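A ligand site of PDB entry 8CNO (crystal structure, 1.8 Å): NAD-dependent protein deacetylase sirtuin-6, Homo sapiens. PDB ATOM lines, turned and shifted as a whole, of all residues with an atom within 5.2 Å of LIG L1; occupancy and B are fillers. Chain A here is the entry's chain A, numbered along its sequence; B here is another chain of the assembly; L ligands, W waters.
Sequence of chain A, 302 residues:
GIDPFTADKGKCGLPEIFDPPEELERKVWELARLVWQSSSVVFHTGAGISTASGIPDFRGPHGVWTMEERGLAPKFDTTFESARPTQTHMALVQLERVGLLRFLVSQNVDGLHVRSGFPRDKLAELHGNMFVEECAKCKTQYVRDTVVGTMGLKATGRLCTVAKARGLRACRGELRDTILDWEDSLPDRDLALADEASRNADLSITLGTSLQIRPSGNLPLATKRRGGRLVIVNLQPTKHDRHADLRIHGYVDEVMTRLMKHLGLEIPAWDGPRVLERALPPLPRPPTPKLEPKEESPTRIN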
ATOM      1  N   GLU A  16      19.937 -25.158  -9.476  1.00  0.00           N
ATOM      2  CA  GLU A  16      21.082 -25.800 -10.188  1.00  0.00           C
ATOM      3  C   GLU A  16      21.755 -26.795  -9.256  1.00  0.00           C
ATOM      4  O   GLU A  16      21.725 -26.640  -8.019  1.00  0.00           O
ATOM      5  CB  GLU A  16      22.087 -24.771 -10.679  1.00  0.00           C
ATOM      6  CG  GLU A  16      21.476 -23.766 -11.623  1.00  0.00           C
ATOM      7  CD  GLU A  16      22.476 -22.835 -12.239  1.00  0.00           C
ATOM      8  OE1 GLU A  16      23.364 -22.344 -11.493  1.00  0.00           O
ATOM      9  OE2 GLU A  16      22.367 -22.584 -13.462  1.00  0.00           O
ATOM     10  N   GLY A  46      20.342 -28.478 -26.422  1.00  0.00           N
ATOM     11  CA  GLY A  46      19.396 -27.381 -26.189  1.00  0.00           C
ATOM     12  C   GLY A  46      20.123 -26.152 -25.724  1.00  0.00           C
ATOM     13  O   GLY A  46      21.336 -25.972 -26.024  1.00  0.00           O
ATOM     14  N   ALA A  47      19.291 -25.213 -25.264  1.00  0.00           N
ATOM     15  CA  ALA A  47      19.618 -23.798 -25.115  1.00  0.00           C
ATOM     16  C   ALA A  47      20.816 -23.637 -24.171  1.00  0.00           C
ATOM     17  O   ALA A  47      21.619 -22.694 -24.383  1.00  0.00           O
ATOM     18  CB  ALA A  47      18.418 -23.054 -24.636  1.00  0.00           C
ATOM     19  N   GLY A  48      21.044 -24.563 -23.251  1.00  0.00           N
ATOM     20  CA  GLY A  48      22.160 -24.456 -22.290  1.00  0.00           C
ATOM     21  C   GLY A  48      23.523 -24.474 -22.974  1.00  0.00           C
ATOM     22  O   GLY A  48      24.480 -24.030 -22.351  1.00  0.00           O
ATOM     23  N   ILE A  49      23.665 -24.984 -24.194  1.00  0.00           N
ATOM     24  CA  ILE A  49      25.007 -25.032 -24.872  1.00  0.00           C
ATOM     25  C   ILE A  49      25.342 -23.661 -25.497  1.00  0.00           C
ATOM     26  O   ILE A  49      26.395 -23.565 -26.151  1.00  0.00           O
ATOM     27  CB  ILE A  49      25.161 -26.190 -25.910  1.00  0.00           C
ATOM     28  CG1 ILE A  49      24.398 -25.908 -27.220  1.00  0.00           C
ATOM     29  CG2 ILE A  49      24.798 -27.550 -25.308  1.00  0.00           C
ATOM     30  CD1 ILE A  49      25.013 -26.637 -28.434  1.00  0.00           C
ATOM     31  N   THR A  51      24.444 -20.525 -23.703  1.00  0.00           N
ATOM     32  CA  THR A  51      24.380 -19.565 -22.570  1.00  0.00           C
ATOM     33  C   THR A  51      25.758 -18.903 -22.489  1.00  0.00           C
ATOM     34  O   THR A  51      25.807 -17.705 -22.237  1.00  0.00           O
ATOM     35  CB  THR A  51      23.879 -20.192 -21.267  1.00  0.00           C
ATOM     36  OG1 THR A  51      24.719 -21.290 -20.907  1.00  0.00           O
ATOM     37  CG2 THR A  51      22.377 -20.506 -21.293  1.00  0.00           C
ATOM     38  N   ALA A  52      26.832 -19.655 -22.749  1.00  0.00           N
ATOM     39  CA  ALA A  52      28.247 -19.212 -22.649  1.00  0.00           C
ATOM     40  C   ALA A  52      28.662 -18.308 -23.826  1.00  0.00           C
ATOM     41  O   ALA A  52      29.769 -17.687 -23.773  1.00  0.00           O
ATOM     42  CB  ALA A  52      29.142 -20.418 -22.511  1.00  0.00           C
ATOM     43  N   ASP A  57      18.997 -19.076 -21.908  1.00  0.00           N
ATOM     44  CA  ASP A  57      18.125 -20.264 -22.108  1.00  0.00           C
ATOM     45  C   ASP A  57      16.671 -19.878 -21.767  1.00  0.00           C
ATOM     46  O   ASP A  57      16.367 -18.664 -21.695  1.00  0.00           O
ATOM     47  CB  ASP A  57      18.721 -21.453 -21.331  1.00  0.00           C
ATOM     48  CG  ASP A  57      18.752 -21.331 -19.811  1.00  0.00           C
ATOM     49  OD1 ASP A  57      17.966 -20.567 -19.228  1.00  0.00           O
ATOM     50  OD2 ASP A  57      19.516 -22.066 -19.213  1.00  0.00           O
ATOM     51  N   PHE A  58      15.803 -20.884 -21.645  1.00  0.00           N
ATOM     52  CA  PHE A  58      14.353 -20.749 -21.421  1.00  0.00           C
ATOM     53  C   PHE A  58      13.984 -21.000 -19.967  1.00  0.00           C
ATOM     54  O   PHE A  58      13.093 -20.225 -19.523  1.00  0.00           O
ATOM     55  CB  PHE A  58      13.608 -21.688 -22.379  1.00  0.00           C
ATOM     56  CG  PHE A  58      13.870 -21.321 -23.805  1.00  0.00           C
ATOM     57  CD1 PHE A  58      13.245 -20.205 -24.316  1.00  0.00           C
ATOM     58  CD2 PHE A  58      14.875 -21.916 -24.542  1.00  0.00           C
ATOM     59  CE1 PHE A  58      13.534 -19.758 -25.600  1.00  0.00           C
ATOM     60  CE2 PHE A  58      15.160 -21.484 -25.820  1.00  0.00           C
ATOM     61  CZ  PHE A  58      14.500 -20.398 -26.331  1.00  0.00           C
ATOM     62  N   ARG A  59      14.533 -22.061 -19.334  1.00  0.00           N
ATOM     63  CA  ARG A  59      14.028 -22.613 -18.041  1.00  0.00           C
ATOM     64  C   ARG A  59      15.109 -22.514 -16.974  1.00  0.00           C
ATOM     65  O   ARG A  59      14.851 -22.950 -15.820  1.00  0.00           O
ATOM     66  CB  ARG A  59      13.418 -23.996 -18.264  1.00  0.00           C
ATOM     67  CG  ARG A  59      12.205 -23.906 -19.166  1.00  0.00           C
ATOM     68  CD  ARG A  59      11.462 -25.204 -19.459  1.00  0.00           C
ATOM     69  NE  ARG A  59      10.485 -25.048 -20.503  1.00  0.00           N
ATOM     70  CZ  ARG A  59      10.710 -24.998 -21.819  1.00  0.00           C
ATOM     71  NH1 ARG A  59      11.937 -25.199 -22.312  1.00  0.00           N
ATOM     72  NH2 ARG A  59       9.691 -24.846 -22.658  1.00  0.00           N
ATOM     73  N   GLY A  60      16.263 -21.916 -17.276  1.00  0.00           N
ATOM     74  CA  GLY A  60      17.318 -21.705 -16.267  1.00  0.00           C
ATOM     75  C   GLY A  60      16.965 -20.583 -15.277  1.00  0.00           C
ATOM     76  O   GLY A  60      15.957 -19.876 -15.412  1.00  0.00           O
ATOM     77  N   TRP A  65      11.551 -17.857 -20.004  1.00  0.00           N
ATOM     78  CA  TRP A  65      10.257 -18.159 -19.339  1.00  0.00           C
ATOM     79  C   TRP A  65      10.374 -17.925 -17.833  1.00  0.00           C
ATOM     80  O   TRP A  65       9.435 -17.345 -17.237  1.00  0.00           O
ATOM     81  CB  TRP A  65       9.714 -19.559 -19.657  1.00  0.00           C
ATOM     82  CG  TRP A  65       9.678 -19.954 -21.110  1.00  0.00           C
ATOM     83  CD1 TRP A  65       9.921 -21.204 -21.592  1.00  0.00           C
ATOM     84  CD2 TRP A  65       9.359 -19.143 -22.257  1.00  0.00           C
ATOM     85  NE1 TRP A  65       9.791 -21.230 -22.949  1.00  0.00           N
ATOM     86  CE2 TRP A  65       9.441 -19.981 -23.390  1.00  0.00           C
ATOM     87  CE3 TRP A  65       9.010 -17.798 -22.451  1.00  0.00           C
ATOM     88  CZ2 TRP A  65       9.218 -19.523 -24.684  1.00  0.00           C
ATOM     89  CZ3 TRP A  65       8.785 -17.337 -23.724  1.00  0.00           C
ATOM     90  CH2 TRP A  65       8.895 -18.186 -24.834  1.00  0.00           C
ATOM     91  N   GLN A 107      17.229 -28.763 -30.426  1.00  0.00           N
ATOM     92  CA  GLN A 107      16.057 -27.877 -30.198  1.00  0.00           C
ATOM     93  C   GLN A 107      16.403 -26.398 -30.446  1.00  0.00           C
ATOM     94  O   GLN A 107      15.503 -25.541 -30.386  1.00  0.00           O
ATOM     95  CB  GLN A 107      15.593 -28.175 -28.766  1.00  0.00           C
ATOM     96  CG  GLN A 107      14.980 -29.558 -28.618  1.00  0.00           C
ATOM     97  CD  GLN A 107      14.724 -29.890 -27.182  1.00  0.00           C
ATOM     98  OE1 GLN A 107      13.776 -29.397 -26.584  1.00  0.00           O
ATOM     99  NE2 GLN A 107      15.616 -30.692 -26.602  1.00  0.00           N
ATOM    100  N   ASN A 108      17.666 -26.050 -30.722  1.00  0.00           N
ATOM    101  CA  ASN A 108      18.057 -24.615 -30.742  1.00  0.00           C
ATOM    102  C   ASN A 108      17.673 -24.012 -32.085  1.00  0.00           C
ATOM    103  O   ASN A 108      18.009 -24.663 -33.126  1.00  0.00           O
ATOM    104  CB  ASN A 108      19.542 -24.456 -30.438  1.00  0.00           C
ATOM    105  CG  ASN A 108      19.882 -24.981 -29.055  1.00  0.00           C
ATOM    106  OD1 ASN A 108      19.009 -25.255 -28.213  1.00  0.00           O
ATOM    107  ND2 ASN A 108      21.162 -25.030 -28.769  1.00  0.00           N
ATOM    108  N   HIS A 127      13.213 -27.357 -34.103  1.00  0.00           N
ATOM    109  CA  HIS A 127      12.334 -26.201 -33.803  1.00  0.00           C
ATOM    110  C   HIS A 127      12.610 -25.086 -34.813  1.00  0.00           C
ATOM    111  O   HIS A 127      11.946 -24.017 -34.719  1.00  0.00           O
ATOM    112  CB  HIS A 127      12.483 -25.744 -32.328  1.00  0.00           C
ATOM    113  CG  HIS A 127      12.258 -26.829 -31.321  1.00  0.00           C
ATOM    114  ND1 HIS A 127      12.517 -26.665 -29.963  1.00  0.00           N
ATOM    115  CD2 HIS A 127      11.791 -28.096 -31.462  1.00  0.00           C
ATOM    116  CE1 HIS A 127      12.271 -27.784 -29.335  1.00  0.00           C
ATOM    117  NE2 HIS A 127      11.781 -28.675 -30.226  1.00  0.00           N
ATOM    118  N   TRP A 182       3.839 -22.544 -31.267  1.00  0.00           N
ATOM    119  CA  TRP A 182       3.402 -23.562 -30.282  1.00  0.00           C
ATOM    120  C   TRP A 182       2.556 -24.648 -30.968  1.00  0.00           C
ATOM    121  O   TRP A 182       2.813 -25.839 -30.685  1.00  0.00           O
ATOM    122  CB  TRP A 182       2.637 -22.885 -29.140  1.00  0.00           C
ATOM    123  CG  TRP A 182       3.516 -22.041 -28.283  1.00  0.00           C
ATOM    124  CD1 TRP A 182       3.639 -20.679 -28.312  1.00  0.00           C
ATOM    125  CD2 TRP A 182       4.447 -22.500 -27.277  1.00  0.00           C
ATOM    126  NE1 TRP A 182       4.554 -20.259 -27.387  1.00  0.00           N
ATOM    127  CE2 TRP A 182       5.072 -21.358 -26.744  1.00  0.00           C
ATOM    128  CE3 TRP A 182       4.805 -23.758 -26.789  1.00  0.00           C
ATOM    129  CZ2 TRP A 182       6.033 -21.442 -25.739  1.00  0.00           C
ATOM    130  CZ3 TRP A 182       5.758 -23.839 -25.798  1.00  0.00           C
ATOM    131  CH2 TRP A 182       6.357 -22.695 -25.277  1.00  0.00           C
ATOM    132  N   GLY A 208      22.776 -29.503 -22.049  1.00  0.00           N
ATOM    133  CA  GLY A 208      22.027 -28.231 -21.855  1.00  0.00           C
ATOM    134  C   GLY A 208      20.626 -28.263 -22.397  1.00  0.00           C
ATOM    135  O   GLY A 208      20.248 -27.277 -23.006  1.00  0.00           O
ATOM    136  N   THR A 209      19.872 -29.359 -22.215  1.00  0.00           N
ATOM    137  CA  THR A 209      18.398 -29.351 -22.412  1.00  0.00           C
ATOM    138  C   THR A 209      17.704 -29.946 -21.174  1.00  0.00           C
ATOM    139  O   THR A 209      18.223 -30.924 -20.597  1.00  0.00           O
ATOM    140  CB  THR A 209      17.973 -30.143 -23.659  1.00  0.00           C
ATOM    141  OG1 THR A 209      16.551 -30.221 -23.599  1.00  0.00           O
ATOM    142  CG2 THR A 209      18.618 -31.520 -23.733  1.00  0.00           C
ATOM    143  N   SER A 210      16.599 -29.341 -20.789  1.00  0.00           N
ATOM    144  CA  SER A 210      15.790 -29.872 -19.662  1.00  0.00           C
ATOM    145  C   SER A 210      14.944 -31.072 -20.134  1.00  0.00           C
ATOM    146  O   SER A 210      14.411 -31.815 -19.231  1.00  0.00           O
ATOM    147  CB  SER A 210      14.964 -28.773 -18.986  1.00  0.00           C
ATOM    148  OG  SER A 210      14.010 -28.169 -19.850  1.00  0.00           O
ATOM    149  N   LEU A 211      14.780 -31.264 -21.450  1.00  0.00           N
ATOM    150  CA  LEU A 211      14.047 -32.446 -22.043  1.00  0.00           C
ATOM    151  C   LEU A 211      12.531 -32.419 -21.748  1.00  0.00           C
ATOM    152  O   LEU A 211      11.872 -33.496 -21.731  1.00  0.00           O
ATOM    153  CB  LEU A 211      14.660 -33.752 -21.554  1.00  0.00           C
ATOM    154  CG  LEU A 211      16.149 -33.905 -21.830  1.00  0.00           C
ATOM    155  CD1 LEU A 211      16.708 -35.203 -21.275  1.00  0.00           C
ATOM    156  CD2 LEU A 211      16.434 -33.777 -23.327  1.00  0.00           C
ATOM    157  N   GLN A 212      11.945 -31.234 -21.616  1.00  0.00           N
ATOM    158  CA  GLN A 212      10.548 -31.042 -21.162  1.00  0.00           C
ATOM    159  C   GLN A 212       9.601 -31.005 -22.374  1.00  0.00           C
ATOM    160  O   GLN A 212       8.396 -31.099 -22.143  1.00  0.00           O
ATOM    161  CB  GLN A 212      10.447 -29.748 -20.377  1.00  0.00           C
ATOM    162  CG  GLN A 212      11.158 -29.800 -19.034  1.00  0.00           C
ATOM    163  CD  GLN A 212      10.765 -28.653 -18.138  1.00  0.00           C
ATOM    164  OE1 GLN A 212       9.575 -28.410 -17.900  1.00  0.00           O
ATOM    165  NE2 GLN A 212      11.761 -28.008 -17.546  1.00  0.00           N
ATOM    166  N   ILE A 213      10.122 -30.798 -23.593  1.00  0.00           N
ATOM    167  CA  ILE A 213       9.313 -30.660 -24.830  1.00  0.00           C
ATOM    168  C   ILE A 213       9.094 -32.059 -25.386  1.00  0.00           C
ATOM    169  O   ILE A 213      10.076 -32.814 -25.488  1.00  0.00           O
ATOM    170  CB  ILE A 213       9.983 -29.735 -25.878  1.00  0.00           C
ATOM    171  CG1 ILE A 213      10.151 -28.297 -25.373  1.00  0.00           C
ATOM    172  CG2 ILE A 213       9.243 -29.787 -27.210  1.00  0.00           C
ATOM    173  CD1 ILE A 213       8.842 -27.579 -25.065  1.00  0.00           C
ATOM    174  N   VAL A 233      23.890 -34.380 -19.543  1.00  0.00           N
ATOM    175  CA  VAL A 233      24.711 -33.267 -18.999  1.00  0.00           C
ATOM    176  C   VAL A 233      23.822 -32.025 -18.879  1.00  0.00           C
ATOM    177  O   VAL A 233      23.317 -31.505 -19.948  1.00  0.00           O
ATOM    178  CB  VAL A 233      25.954 -33.044 -19.886  1.00  0.00           C
ATOM    179  CG1 VAL A 233      26.925 -32.008 -19.307  1.00  0.00           C
ATOM    180  CG2 VAL A 233      26.694 -34.341 -20.214  1.00  0.00           C
ATOM    181  N   ASN A 234      23.650 -31.500 -17.660  1.00  0.00           N
ATOM    182  CA  ASN A 234      22.712 -30.371 -17.371  1.00  0.00           C
ATOM    183  C   ASN A 234      22.929 -29.843 -15.962  1.00  0.00           C
ATOM    184  O   ASN A 234      23.094 -30.682 -15.009  1.00  0.00           O
ATOM    185  CB  ASN A 234      21.270 -30.805 -17.630  1.00  0.00           C
ATOM    186  CG  ASN A 234      20.420 -29.633 -18.036  1.00  0.00           C
ATOM    187  OD1 ASN A 234      20.700 -28.968 -19.032  1.00  0.00           O
ATOM    188  ND2 ASN A 234      19.390 -29.365 -17.286  1.00  0.00           N
ATOM    189  N   LEU A 235      22.862 -28.526 -15.811  1.00  0.00           N
ATOM    190  CA  LEU A 235      23.006 -27.866 -14.490  1.00  0.00           C
ATOM    191  C   LEU A 235      21.737 -28.108 -13.653  1.00  0.00           C
ATOM    192  O   LEU A 235      21.897 -28.371 -12.441  1.00  0.00           O
ATOM    193  CB  LEU A 235      23.332 -26.400 -14.715  1.00  0.00           C
ATOM    194  CG  LEU A 235      24.803 -26.135 -15.031  1.00  0.00           C
ATOM    195  CD1 LEU A 235      25.009 -24.667 -15.383  1.00  0.00           C
ATOM    196  CD2 LEU A 235      25.700 -26.519 -13.856  1.00  0.00           C
ATOM    197  N   GLN A 236      20.548 -28.133 -14.260  1.00  0.00           N
ATOM    198  CA  GLN A 236      19.262 -28.382 -13.569  1.00  0.00           C
ATOM    199  C   GLN A 236      18.863 -29.858 -13.708  1.00  0.00           C
ATOM    200  O   GLN A 236      19.367 -30.579 -14.567  1.00  0.00           O
ATOM    201  CB  GLN A 236      18.137 -27.530 -14.162  1.00  0.00           C
ATOM    202  CG  GLN A 236      18.147 -26.081 -13.720  1.00  0.00           C
ATOM    203  CD  GLN A 236      17.110 -25.251 -14.455  1.00  0.00           C
ATOM    204  OE1 GLN A 236      16.750 -25.508 -15.598  1.00  0.00           O
ATOM    205  NE2 GLN A 236      16.597 -24.220 -13.787  1.00  0.00           N
ATOM    206  N   PRO A 237      17.971 -30.356 -12.830  1.00  0.00           N
ATOM    207  CA  PRO A 237      17.240 -31.599 -13.107  1.00  0.00           C
ATOM    208  C   PRO A 237      16.548 -31.536 -14.471  1.00  0.00           C
ATOM    209  O   PRO A 237      16.168 -30.485 -14.898  1.00  0.00           O
ATOM    210  CB  PRO A 237      16.192 -31.634 -11.952  1.00  0.00           C
ATOM    211  CG  PRO A 237      16.837 -30.818 -10.852  1.00  0.00           C
ATOM    212  CD  PRO A 237      17.463 -29.682 -11.620  1.00  0.00           C
ATOM    213  N   GLY A 250      27.309 -29.959 -14.416  1.00  0.00           N
ATOM    214  CA  GLY A 250      28.396 -28.967 -14.490  1.00  0.00           C
ATOM    215  C   GLY A 250      28.161 -28.187 -15.737  1.00  0.00           C
ATOM    216  O   GLY A 250      27.232 -28.589 -16.463  1.00  0.00           O
ATOM    217  N   TYR A 251      28.991 -27.186 -15.980  1.00  0.00           N
ATOM    218  CA  TYR A 251      28.973 -26.349 -17.212  1.00  0.00           C
ATOM    219  C   TYR A 251      29.393 -27.215 -18.401  1.00  0.00           C
ATOM    220  O   TYR A 251      30.427 -27.973 -18.297  1.00  0.00           O
ATOM    221  CB  TYR A 251      29.876 -25.136 -17.026  1.00  0.00           C
ATOM    222  CG  TYR A 251      29.382 -24.178 -15.979  1.00  0.00           C
ATOM    223  CD1 TYR A 251      28.405 -23.242 -16.291  1.00  0.00           C
ATOM    224  CD2 TYR A 251      29.899 -24.170 -14.697  1.00  0.00           C
ATOM    225  CE1 TYR A 251      27.950 -22.331 -15.370  1.00  0.00           C
ATOM    226  CE2 TYR A 251      29.419 -23.297 -13.728  1.00  0.00           C
ATOM    227  CZ  TYR A 251      28.459 -22.354 -14.075  1.00  0.00           C
ATOM    228  OH  TYR A 251      27.994 -21.493 -13.158  1.00  0.00           O
ATOM    229  N   VAL A 252      28.577 -27.233 -19.469  1.00  0.00           N
ATOM    230  CA  VAL A 252      28.793 -28.135 -20.629  1.00  0.00           C
ATOM    231  C   VAL A 252      30.175 -27.893 -21.241  1.00  0.00           C
ATOM    232  O   VAL A 252      30.839 -28.877 -21.555  1.00  0.00           O
ATOM    233  CB  VAL A 252      27.653 -28.077 -21.659  1.00  0.00           C
ATOM    234  CG1 VAL A 252      27.465 -26.717 -22.293  1.00  0.00           C
ATOM    235  CG2 VAL A 252      27.828 -29.138 -22.713  1.00  0.00           C
ATOM    236  N   ASP B  77      27.465 -18.340 -16.583  1.00  0.00           N
ATOM    237  CA  ASP B  77      27.256 -19.429 -17.592  1.00  0.00           C
ATOM    238  C   ASP B  77      28.587 -20.177 -17.816  1.00  0.00           C
ATOM    239  O   ASP B  77      28.621 -21.024 -18.681  1.00  0.00           O
ATOM    240  CB  ASP B  77      26.700 -18.844 -18.888  1.00  0.00           C
ATOM    241  CG  ASP B  77      25.451 -17.979 -18.702  1.00  0.00           C
ATOM    242  OD1 ASP B  77      24.395 -18.511 -18.249  1.00  0.00           O
ATOM    243  OD2 ASP B  77      25.525 -16.795 -18.972  1.00  0.00           O
HETATM  244  N1  LIG L   1      26.036 -25.847 -18.961  1.00  0.00           N
HETATM  245  C1  LIG L   1      25.137 -26.801 -18.663  1.00  0.00           C
HETATM  246  N2  LIG L   1      23.809 -26.734 -18.562  1.00  0.00           N
HETATM  247  C2  LIG L   1      23.384 -25.506 -18.863  1.00  0.00           C
HETATM  248  C3  LIG L   1      24.173 -24.418 -19.154  1.00  0.00           C
HETATM  249  C4  LIG L   1      25.574 -24.603 -19.231  1.00  0.00           C
HETATM  250  N3  LIG L   1      26.420 -23.650 -19.567  1.00  0.00           N
HETATM  251  N4  LIG L   1      23.371 -23.328 -19.395  1.00  0.00           N
HETATM  252  C5  LIG L   1      22.137 -23.744 -19.175  1.00  0.00           C
HETATM  253  N5  LIG L   1      22.087 -25.045 -18.860  1.00  0.00           N
HETATM  254  P1  LIG L   1      15.670 -25.152 -21.377  1.00  0.00           P
HETATM  255  P2  LIG L   1      15.581 -26.353 -24.022  1.00  0.00           P
HETATM  256  C6  LIG L   1      20.913 -25.867 -18.704  1.00  0.00           C
HETATM  257  O1  LIG L   1      14.387 -25.799 -20.978  1.00  0.00           O
HETATM  258  O2  LIG L   1      16.446 -26.202 -25.266  1.00  0.00           O
HETATM  259  C7  LIG L   1      11.463 -23.668 -25.651  1.00  0.00           C
HETATM  260  O3  LIG L   1      10.119 -23.226 -25.483  1.00  0.00           O
HETATM  261  C8  LIG L   1      19.833 -25.327 -17.800  1.00  0.00           C
HETATM  262  O4  LIG L   1      19.934 -25.801 -16.467  1.00  0.00           O
HETATM  263  O5  LIG L   1      16.026 -23.775 -20.916  1.00  0.00           O
HETATM  264  O6  LIG L   1      15.657 -27.644 -23.305  1.00  0.00           O
HETATM  265  C9  LIG L   1      12.050 -23.581 -27.065  1.00  0.00           C
HETATM  266  O7  LIG L   1      11.212 -24.105 -28.087  1.00  0.00           O
HETATM  267  C10 LIG L   1      18.553 -25.869 -18.453  1.00  0.00           C
HETATM  268  O8  LIG L   1      17.934 -26.842 -17.638  1.00  0.00           O
HETATM  269  O9  LIG L   1      16.006 -25.200 -22.963  1.00  0.00           O
HETATM  270  C11 LIG L   1      13.208 -24.578 -26.949  1.00  0.00           C
HETATM  271  O10 LIG L   1      13.743 -24.908 -28.223  1.00  0.00           O
HETATM  272  C12 LIG L   1      18.964 -26.310 -19.867  1.00  0.00           C
HETATM  273  O11 LIG L   1      20.373 -25.965 -20.004  1.00  0.00           O
HETATM  274  C13 LIG L   1      12.525 -25.709 -26.174  1.00  0.00           C
HETATM  275  O12 LIG L   1      11.584 -25.030 -25.310  1.00  0.00           O
HETATM  276  C14 LIG L   1      18.172 -25.581 -20.921  1.00  0.00           C
HETATM  277  O13 LIG L   1      16.809 -26.104 -20.864  1.00  0.00           O
HETATM  278  C15 LIG L   1      13.395 -26.613 -25.365  1.00  0.00           C
HETATM  279  O14 LIG L   1      14.150 -25.836 -24.390  1.00  0.00           O
HETATM  280  C1  LG2 L   2      16.441 -17.310 -26.576  1.00  0.00           C
HETATM  281  C2  LG2 L   2      17.246 -18.281 -27.203  1.00  0.00           C
HETATM  282  C3  LG2 L   2      17.058 -18.624 -28.561  1.00  0.00           C
HETATM  283  C4  LG2 L   2      16.072 -17.955 -29.315  1.00  0.00           C
HETATM  284  C5  LG2 L   2      15.234 -16.993 -28.718  1.00  0.00           C
HETATM  285  C6  LG2 L   2      15.423 -16.680 -27.319  1.00  0.00           C
HETATM  286  C7  LG2 L   2      14.210 -16.349 -29.495  1.00  0.00           C
HETATM  287  C8  LG2 L   2      13.113 -16.919 -30.143  1.00  0.00           C
HETATM  288  C9  LG2 L   2      12.656 -18.231 -30.278  1.00  0.00           C
HETATM  289  C10 LG2 L   2      12.960 -19.175 -29.256  1.00  0.00           C
HETATM  290  C11 LG2 L   2      12.568 -20.528 -29.288  1.00  0.00           C
HETATM  291  C12 LG2 L   2      11.777 -21.017 -30.337  1.00  0.00           C
HETATM  292  C13 LG2 L   2      11.413 -20.092 -31.335  1.00  0.00           C
HETATM  293  C14 LG2 L   2      11.834 -18.740 -31.300  1.00  0.00           C
HETATM  294  O1  LG2 L   2      11.410 -22.336 -30.316  1.00  0.00           O
HETATM  295  O2  LG2 L   2      17.810 -19.561 -29.185  1.00  0.00           O
HETATM  296  O3  LG2 L   2      16.633 -17.014 -25.271  1.00  0.00           O
HETATM  297  O   HOH W   1      16.490 -24.700 -27.431  1.00  0.00           O
HETATM  298  O   HOH W   2      20.775 -21.383 -17.061  1.00  0.00           O
HETATM  299  O   HOH W   3      26.953 -22.618 -22.616  1.00  0.00           O
HETATM  300  O   HOH W   4      13.108 -28.621 -22.539  1.00  0.00           O
HETATM  301  O   HOH W   5      23.730 -21.298 -17.514  1.00  0.00           O
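NE2 of Gln 236 sits at hydrogen-bond distance from O of Arg 59 (3.0 Å).
NE2 of Gln 107 is in hydrogen-bond range of OG1 of Thr 209 (3.2 Å).
N of Thr 209 sits at hydrogen-bond distance from OD1 of Asn 234, 3.3 Å away.
A ring nitrogen (ND1) of His 127 lies within hydrogen-bond range of the backbone carbonyl oxygen (O) of Gln 107 (3.2 Å).
O of Phe 58 sits at hydrogen-bond distance from N of Trp 65, 2.9 Å away.
The backbone carbonyl oxygen (O) of Gly 208 lies within hydrogen-bond range of the backbone NH (N) of Ala 47 (3.2 Å).
OD1 of Asp 57 lies within hydrogen-bond range of N of Gly 60, at 2.9 Å.
The backbone NH (N) of Gly 48 sits at hydrogen-bond distance from the backbone carbonyl oxygen (O) of Gly 208, 2.8 Å away.
The backbone NH (N) of Ser 210 is in hydrogen-bond range of an oxygen (O6) of LIG L1 (3.2 Å).
An oxygen (O1) of LIG L1 lies within hydrogen-bond range of the side-chain hydroxyl (OG) of Ser 210 (2.7 Å).
The backbone NH (N) of Gln 236 is in hydrogen-bond range of an oxygen (O4) of LIG L1 (3.3 Å).
OE1 of Gln 236 lies within hydrogen-bond range of O8 of LIG L1.
The side-chain hydroxyl of Thr 209 lies within hydrogen-bond range of an oxygen (O6) of LIG L1 (2.7 Å).
A ring nitrogen (ND1) of His 127 sits at hydrogen-bond distance from an oxygen (O10) of LIG L1, at 2.8 Å.
The backbone NH (N) of Arg 59 sits at hydrogen-bond distance from an oxygen (O5) of LIG L1 (2.8 Å).
An oxygen (O1) of LIG L1 is in salt-bridge range of the guanidinium group of Arg 59.
The backbone carbonyl oxygen (O) of Gln 107 is in hydrogen-bond range of an oxygen (O10) of LIG L1 (2.9 Å).
A nitrogen (N4) of LIG L1 sits at hydrogen-bond distance from the side-chain hydroxyl (OG1) of Thr 51.
The side-chain amide nitrogen (ND2) of Asn 234 is in hydrogen-bond range of an oxygen (O8) of LIG L1, 2.9 Å away.
A nitrogen (N1) of LIG L1 lies within hydrogen-bond range of the backbone NH (N) of Val 252 (2.9 Å).
N of Phe 58 is in hydrogen-bond range of O5 of LIG L1, at 3.0 Å.
The backbone NH of Ala 47 lies within hydrogen-bond range of an oxygen (O2) of LIG L1 (3.0 Å).
O of Gly 48 lies close to N3 of LIG L1 (3.4 Å).
The indole nitrogen (NE1) of Trp 65 sits at hydrogen-bond distance from an oxygen (O3) of LIG L1 (3.2 Å).
N of Leu 235 is in hydrogen-bond range of N2 of LIG L1.
An oxygen (O7) of LIG L1 is in hydrogen-bond range of an oxygen (O1) of LG2 L2 (2.9 Å).
Water W1 lies within hydrogen-bond range of O2 of LIG L1 (2.6 Å), OD1 of Asn 108 (2.7 Å) and O of Gln 107 (3.2 Å).
Water W5 bridges a nitrogen (N4) of LIG L1 (2.8 Å) and the side-chain carboxylate (OD1) of Asp 77 of chain B (3.0 Å).
Water W4 lies within hydrogen-bond range of O6 of LIG L1 (2.8 Å), OG of Ser 210 (2.9 Å), N of Gln 212 (3.0 Å) and N of Leu 211 (3.3 Å).
Water W3 lies within hydrogen-bond range of O of Gly 48 (2.9 Å), N of Ala 52 (3.0 Å), OG1 of Thr 51 (3.1 Å) and N3 of LIG L1 (3.3 Å).
An oxygen (O11) of LIG L1 sits close to the backbone carbonyl oxygen (O) of Gly 208, 3.3 Å away.
Gly 46 touches LIG L1 (CA to O2, 3.3 Å).
Asp 57 touches LIG L1.
Trp 182 touches LIG L1 (CH2 to O3, 3.8 Å).
CG1 of Ile 213 touches O12 of LIG L1, at 3.6 Å.
Gly 250 touches LIG L1.
CA of Tyr 251 touches N1 of LIG L1, at 3.5 Å.
Asp 77 of chain B touches LIG L1 (O to N3, 3.5 Å).
Of the 31 residues printed, 22 come within 4 Å of LIG L1.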
